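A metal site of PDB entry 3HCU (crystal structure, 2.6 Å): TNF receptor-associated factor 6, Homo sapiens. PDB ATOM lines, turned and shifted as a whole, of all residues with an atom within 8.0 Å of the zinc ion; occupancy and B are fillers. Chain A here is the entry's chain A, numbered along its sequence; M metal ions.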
ATOM      1  N   GLN A   5     -28.308  25.524 -22.189  1.00  0.00           N
ATOM      2  CA  GLN A   5     -29.124  24.284 -22.057  1.00  0.00           C
ATOM      3  C   GLN A   5     -29.800  24.138 -20.675  1.00  0.00           C
ATOM      4  O   GLN A   5     -30.217  23.053 -20.278  1.00  0.00           O
ATOM      5  CB  GLN A   5     -28.253  23.058 -22.386  1.00  0.00           C
ATOM      6  CG  GLN A   5     -28.939  21.982 -23.245  1.00  0.00           C
ATOM      7  CD  GLN A   5     -29.351  22.495 -24.641  1.00  0.00           C
ATOM      8  OE1 GLN A   5     -28.561  23.121 -25.369  1.00  0.00           O
ATOM      9  NE2 GLN A   5     -30.602  22.216 -25.021  1.00  0.00           N
ATOM     10  N   GLY A   6     -29.910  25.228 -19.929  1.00  0.00           N
ATOM     11  CA  GLY A   6     -30.592  25.149 -18.650  1.00  0.00           C
ATOM     12  C   GLY A   6     -32.059  25.341 -18.960  1.00  0.00           C
ATOM     13  O   GLY A   6     -32.438  25.139 -20.109  1.00  0.00           O
ATOM     14  N   TYR A   7     -32.888  25.707 -17.979  1.00  0.00           N
ATOM     15  CA  TYR A   7     -34.312  25.928 -18.255  1.00  0.00           C
ATOM     16  C   TYR A   7     -34.503  27.386 -18.632  1.00  0.00           C
ATOM     17  O   TYR A   7     -34.458  28.275 -17.786  1.00  0.00           O
ATOM     18  CB  TYR A   7     -35.225  25.616 -17.052  1.00  0.00           C
ATOM     19  CG  TYR A   7     -35.225  24.182 -16.517  1.00  0.00           C
ATOM     20  CD1 TYR A   7     -34.327  23.810 -15.523  1.00  0.00           C
ATOM     21  CD2 TYR A   7     -36.111  23.212 -17.009  1.00  0.00           C
ATOM     22  CE1 TYR A   7     -34.288  22.530 -15.028  1.00  0.00           C
ATOM     23  CE2 TYR A   7     -36.078  21.909 -16.507  1.00  0.00           C
ATOM     24  CZ  TYR A   7     -35.138  21.585 -15.522  1.00  0.00           C
ATOM     25  OH  TYR A   7     -35.004  20.305 -15.027  1.00  0.00           O
ATOM     26  N   TYR A  19     -29.503  29.303  -7.910  1.00  0.00           N
ATOM     27  CA  TYR A  19     -29.919  28.286  -8.874  1.00  0.00           C
ATOM     28  C   TYR A  19     -29.621  28.636 -10.333  1.00  0.00           C
ATOM     29  O   TYR A  19     -30.065  27.940 -11.232  1.00  0.00           O
ATOM     30  CB  TYR A  19     -31.418  27.998  -8.752  1.00  0.00           C
ATOM     31  CG  TYR A  19     -31.840  27.452  -7.433  1.00  0.00           C
ATOM     32  CD1 TYR A  19     -31.070  26.500  -6.778  1.00  0.00           C
ATOM     33  CD2 TYR A  19     -33.044  27.855  -6.847  1.00  0.00           C
ATOM     34  CE1 TYR A  19     -31.475  25.943  -5.582  1.00  0.00           C
ATOM     35  CE2 TYR A  19     -33.467  27.324  -5.656  1.00  0.00           C
ATOM     36  CZ  TYR A  19     -32.688  26.354  -5.023  1.00  0.00           C
ATOM     37  OH  TYR A  19     -33.136  25.768  -3.860  1.00  0.00           O
ATOM     38  N   GLU A  20     -28.882  29.713 -10.563  1.00  0.00           N
ATOM     39  CA  GLU A  20     -28.561  30.093 -11.930  1.00  0.00           C
ATOM     40  C   GLU A  20     -27.221  29.499 -12.307  1.00  0.00           C
ATOM     41  O   GLU A  20     -26.277  29.506 -11.523  1.00  0.00           O
ATOM     42  CB  GLU A  20     -28.474  31.605 -12.079  1.00  0.00           C
ATOM     43  CG  GLU A  20     -28.036  32.058 -13.473  1.00  0.00           C
ATOM     44  CD  GLU A  20     -27.858  33.558 -13.551  1.00  0.00           C
ATOM     45  OE1 GLU A  20     -26.759  34.047 -13.208  1.00  0.00           O
ATOM     46  OE2 GLU A  20     -28.839  34.242 -13.937  1.00  0.00           O
ATOM     47  N   CYS A  21     -27.146  29.002 -13.532  1.00  0.00           N
ATOM     48  CA  CYS A  21     -25.937  28.398 -14.033  1.00  0.00           C
ATOM     49  C   CYS A  21     -24.981  29.492 -14.501  1.00  0.00           C
ATOM     50  O   CYS A  21     -25.343  30.320 -15.335  1.00  0.00           O
ATOM     51  CB  CYS A  21     -26.307  27.485 -15.182  1.00  0.00           C
ATOM     52  SG  CYS A  21     -24.935  26.780 -16.055  1.00  0.00           S
ATOM     53  N   PRO A  22     -23.740  29.500 -13.974  1.00  0.00           N
ATOM     54  CA  PRO A  22     -22.767  30.514 -14.382  1.00  0.00           C
ATOM     55  C   PRO A  22     -22.485  30.431 -15.877  1.00  0.00           C
ATOM     56  O   PRO A  22     -22.216  31.441 -16.513  1.00  0.00           O
ATOM     57  CB  PRO A  22     -21.540  30.156 -13.563  1.00  0.00           C
ATOM     58  CG  PRO A  22     -22.085  29.505 -12.380  1.00  0.00           C
ATOM     59  CD  PRO A  22     -23.150  28.617 -12.954  1.00  0.00           C
ATOM     60  N   ILE A  23     -22.562  29.229 -16.427  1.00  0.00           N
ATOM     61  CA  ILE A  23     -22.270  29.055 -17.834  1.00  0.00           C
ATOM     62  C   ILE A  23     -23.367  29.357 -18.843  1.00  0.00           C
ATOM     63  O   ILE A  23     -23.056  29.812 -19.936  1.00  0.00           O
ATOM     64  CB  ILE A  23     -21.716  27.649 -18.109  1.00  0.00           C
ATOM     65  CG1 ILE A  23     -20.415  27.468 -17.331  1.00  0.00           C
ATOM     66  CG2 ILE A  23     -21.485  27.467 -19.624  1.00  0.00           C
ATOM     67  CD1 ILE A  23     -19.787  26.114 -17.482  1.00  0.00           C
ATOM     68  N   CYS A  24     -24.634  29.106 -18.504  1.00  0.00           N
ATOM     69  CA  CYS A  24     -25.696  29.426 -19.465  1.00  0.00           C
ATOM     70  C   CYS A  24     -26.715  30.450 -18.948  1.00  0.00           C
ATOM     71  O   CYS A  24     -27.584  30.898 -19.700  1.00  0.00           O
ATOM     72  CB  CYS A  24     -26.421  28.163 -19.896  1.00  0.00           C
ATOM     73  SG  CYS A  24     -27.525  27.530 -18.675  1.00  0.00           S
ATOM     74  N   LEU A  25     -26.595  30.812 -17.673  1.00  0.00           N
ATOM     75  CA  LEU A  25     -27.468  31.803 -17.041  1.00  0.00           C
ATOM     76  C   LEU A  25     -28.960  31.448 -17.036  1.00  0.00           C
ATOM     77  O   LEU A  25     -29.821  32.330 -17.105  1.00  0.00           O
ATOM     78  CB  LEU A  25     -27.251  33.163 -17.689  1.00  0.00           C
ATOM     79  CG  LEU A  25     -25.973  33.867 -17.231  1.00  0.00           C
ATOM     80  CD1 LEU A  25     -24.916  32.859 -16.813  1.00  0.00           C
ATOM     81  CD2 LEU A  25     -25.462  34.729 -18.367  1.00  0.00           C
ATOM     82  N   MET A  26     -29.232  30.158 -16.950  1.00  0.00           N
ATOM     83  CA  MET A  26     -30.594  29.641 -16.897  1.00  0.00           C
ATOM     84  C   MET A  26     -30.706  28.844 -15.605  1.00  0.00           C
ATOM     85  O   MET A  26     -29.688  28.601 -14.943  1.00  0.00           O
ATOM     86  CB  MET A  26     -30.845  28.716 -18.083  1.00  0.00           C
ATOM     87  CG  MET A  26     -30.542  29.330 -19.447  1.00  0.00           C
ATOM     88  SD  MET A  26     -31.564  30.773 -19.787  1.00  0.00           S
ATOM     89  CE  MET A  26     -30.493  31.705 -20.937  1.00  0.00           C
ATOM     90  N   ALA A  27     -31.913  28.456 -15.212  1.00  0.00           N
ATOM     91  CA  ALA A  27     -32.030  27.661 -13.991  1.00  0.00           C
ATOM     92  C   ALA A  27     -31.267  26.328 -14.187  1.00  0.00           C
ATOM     93  O   ALA A  27     -31.364  25.706 -15.232  1.00  0.00           O
ATOM     94  CB  ALA A  27     -33.468  27.420 -13.701  1.00  0.00           C
ATOM     95  N   LEU A  28     -30.525  25.886 -13.183  1.00  0.00           N
ATOM     96  CA  LEU A  28     -29.759  24.637 -13.312  1.00  0.00           C
ATOM     97  C   LEU A  28     -30.592  23.440 -13.796  1.00  0.00           C
ATOM     98  O   LEU A  28     -31.575  23.078 -13.171  1.00  0.00           O
ATOM     99  CB  LEU A  28     -29.085  24.288 -11.974  1.00  0.00           C
ATOM    100  CG  LEU A  28     -28.126  25.273 -11.317  1.00  0.00           C
ATOM    101  CD1 LEU A  28     -27.688  24.707  -9.989  1.00  0.00           C
ATOM    102  CD2 LEU A  28     -26.929  25.560 -12.196  1.00  0.00           C
ATOM    103  N   ARG A  29     -30.178  22.825 -14.902  1.00  0.00           N
ATOM    104  CA  ARG A  29     -30.853  21.646 -15.447  1.00  0.00           C
ATOM    105  C   ARG A  29     -29.978  20.428 -15.101  1.00  0.00           C
ATOM    106  O   ARG A  29     -28.839  20.314 -15.572  1.00  0.00           O
ATOM    107  CB  ARG A  29     -31.034  21.757 -16.976  1.00  0.00           C
ATOM    108  CG  ARG A  29     -31.803  20.574 -17.592  1.00  0.00           C
ATOM    109  CD  ARG A  29     -31.643  20.476 -19.099  1.00  0.00           C
ATOM    110  NE  ARG A  29     -32.326  21.547 -19.806  1.00  0.00           N
ATOM    111  CZ  ARG A  29     -33.641  21.618 -19.955  1.00  0.00           C
ATOM    112  NH1 ARG A  29     -34.434  20.673 -19.460  1.00  0.00           N
ATOM    113  NH2 ARG A  29     -34.180  22.658 -20.576  1.00  0.00           N
ATOM    114  N   ARG A  39     -22.213  25.171  -8.559  1.00  0.00           N
ATOM    115  CA  ARG A  39     -23.258  24.442  -9.263  1.00  0.00           C
ATOM    116  C   ARG A  39     -23.350  24.855 -10.731  1.00  0.00           C
ATOM    117  O   ARG A  39     -23.126  26.019 -11.081  1.00  0.00           O
ATOM    118  CB  ARG A  39     -24.602  24.707  -8.586  1.00  0.00           C
ATOM    119  CG  ARG A  39     -24.659  24.427  -7.102  1.00  0.00           C
ATOM    120  CD  ARG A  39     -26.005  24.918  -6.572  1.00  0.00           C
ATOM    121  NE  ARG A  39     -26.430  24.190  -5.380  1.00  0.00           N
ATOM    122  CZ  ARG A  39     -25.910  24.362  -4.173  1.00  0.00           C
ATOM    123  NH1 ARG A  39     -24.962  25.257  -3.980  1.00  0.00           N
ATOM    124  NH2 ARG A  39     -26.324  23.608  -3.161  1.00  0.00           N
ATOM    125  N   PHE A  40     -23.684  23.883 -11.572  1.00  0.00           N
ATOM    126  CA  PHE A  40     -23.840  24.070 -13.001  1.00  0.00           C
ATOM    127  C   PHE A  40     -24.942  23.142 -13.474  1.00  0.00           C
ATOM    128  O   PHE A  40     -25.475  22.345 -12.688  1.00  0.00           O
ATOM    129  CB  PHE A  40     -22.550  23.679 -13.763  1.00  0.00           C
ATOM    130  CG  PHE A  40     -21.329  24.468 -13.397  1.00  0.00           C
ATOM    131  CD1 PHE A  40     -20.373  23.936 -12.535  1.00  0.00           C
ATOM    132  CD2 PHE A  40     -21.137  25.751 -13.896  1.00  0.00           C
ATOM    133  CE1 PHE A  40     -19.260  24.679 -12.169  1.00  0.00           C
ATOM    134  CE2 PHE A  40     -20.023  26.494 -13.531  1.00  0.00           C
ATOM    135  CZ  PHE A  40     -19.081  25.946 -12.660  1.00  0.00           C
ATOM    136  N   CYS A  41     -25.304  23.244 -14.740  1.00  0.00           N
ATOM    137  CA  CYS A  41     -26.250  22.278 -15.305  1.00  0.00           C
ATOM    138  C   CYS A  41     -25.301  21.124 -15.644  1.00  0.00           C
ATOM    139  O   CYS A  41     -24.233  21.375 -16.181  1.00  0.00           O
ATOM    140  CB  CYS A  41     -26.851  22.752 -16.631  1.00  0.00           C
ATOM    141  SG  CYS A  41     -27.736  24.275 -16.638  1.00  0.00           S
ATOM    142  N   LYS A  42     -25.674  19.902 -15.327  1.00  0.00           N
ATOM    143  CA  LYS A  42     -24.864  18.711 -15.635  1.00  0.00           C
ATOM    144  C   LYS A  42     -24.212  18.814 -17.010  1.00  0.00           C
ATOM    145  O   LYS A  42     -23.031  18.512 -17.172  1.00  0.00           O
ATOM    146  CB  LYS A  42     -25.779  17.491 -15.588  1.00  0.00           C
ATOM    147  CG  LYS A  42     -25.248  16.208 -16.211  1.00  0.00           C
ATOM    148  CD  LYS A  42     -24.432  15.387 -15.235  1.00  0.00           C
ATOM    149  CE  LYS A  42     -24.492  13.911 -15.612  1.00  0.00           C
ATOM    150  NZ  LYS A  42     -25.912  13.432 -15.660  1.00  0.00           N
ATOM    151  N   ALA A  43     -24.975  19.264 -18.019  1.00  0.00           N
ATOM    152  CA  ALA A  43     -24.461  19.376 -19.383  1.00  0.00           C
ATOM    153  C   ALA A  43     -23.548  20.544 -19.624  1.00  0.00           C
ATOM    154  O   ALA A  43     -22.778  20.545 -20.579  1.00  0.00           O
ATOM    155  CB  ALA A  43     -25.621  19.442 -20.374  1.00  0.00           C
ATOM    156  N   CYS A  44     -23.624  21.570 -18.784  1.00  0.00           N
ATOM    157  CA  CYS A  44     -22.765  22.721 -19.014  1.00  0.00           C
ATOM    158  C   CYS A  44     -21.339  22.544 -18.481  1.00  0.00           C
ATOM    159  O   CYS A  44     -20.367  22.944 -19.139  1.00  0.00           O
ATOM    160  CB  CYS A  44     -23.402  23.993 -18.419  1.00  0.00           C
ATOM    161  SG  CYS A  44     -24.784  24.723 -19.375  1.00  0.00           S
ATOM    162  N   ILE A  45     -21.178  21.945 -17.310  1.00  0.00           N
ATOM    163  CA  ILE A  45     -19.835  21.814 -16.803  1.00  0.00           C
ATOM    164  C   ILE A  45     -19.075  20.730 -17.572  1.00  0.00           C
ATOM    165  O   ILE A  45     -17.837  20.731 -17.606  1.00  0.00           O
ATOM    166  CB  ILE A  45     -19.844  21.569 -15.293  1.00  0.00           C
ATOM    167  CG1 ILE A  45     -18.487  21.940 -14.712  1.00  0.00           C
ATOM    168  CG2 ILE A  45     -20.187  20.129 -15.001  1.00  0.00           C
ATOM    169  CD1 ILE A  45     -18.129  23.405 -14.947  1.00  0.00           C
HETATM  170 ZN    ZN M   1     -26.213  25.650 -17.658  1.00  0.00          ZN
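The backbone NH (N) of Cys 21 is in hydrogen-bond range of the backbone carbonyl oxygen (O) of Met 26 (2.9 Å). The side-chain sulfur of Cys 24 lies close to the backbone NH of Gly 6, 3.5 Å away. SG of Cys 21 sits close to N of Ile 23 (3.4 Å). SG of Cys 41 sits close to N of Arg 29, 3.3 Å away. N of Met 26 lies close to SG of Cys 24.
Within 4 Å of the zinc ion: Cys 21, Cys 24, Cys 41 and Cys 44.
The zinc ion is bound by the side-chain sulfur of Cys 41 (2.3 Å), the side-chain sulfur of Cys 21 (2.3 Å), the side-chain sulfur of Cys 44 (2.4 Å) and the side-chain sulfur of Cys 24 (2.5 Å). The zinc ion has four donor atoms within binding distance.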
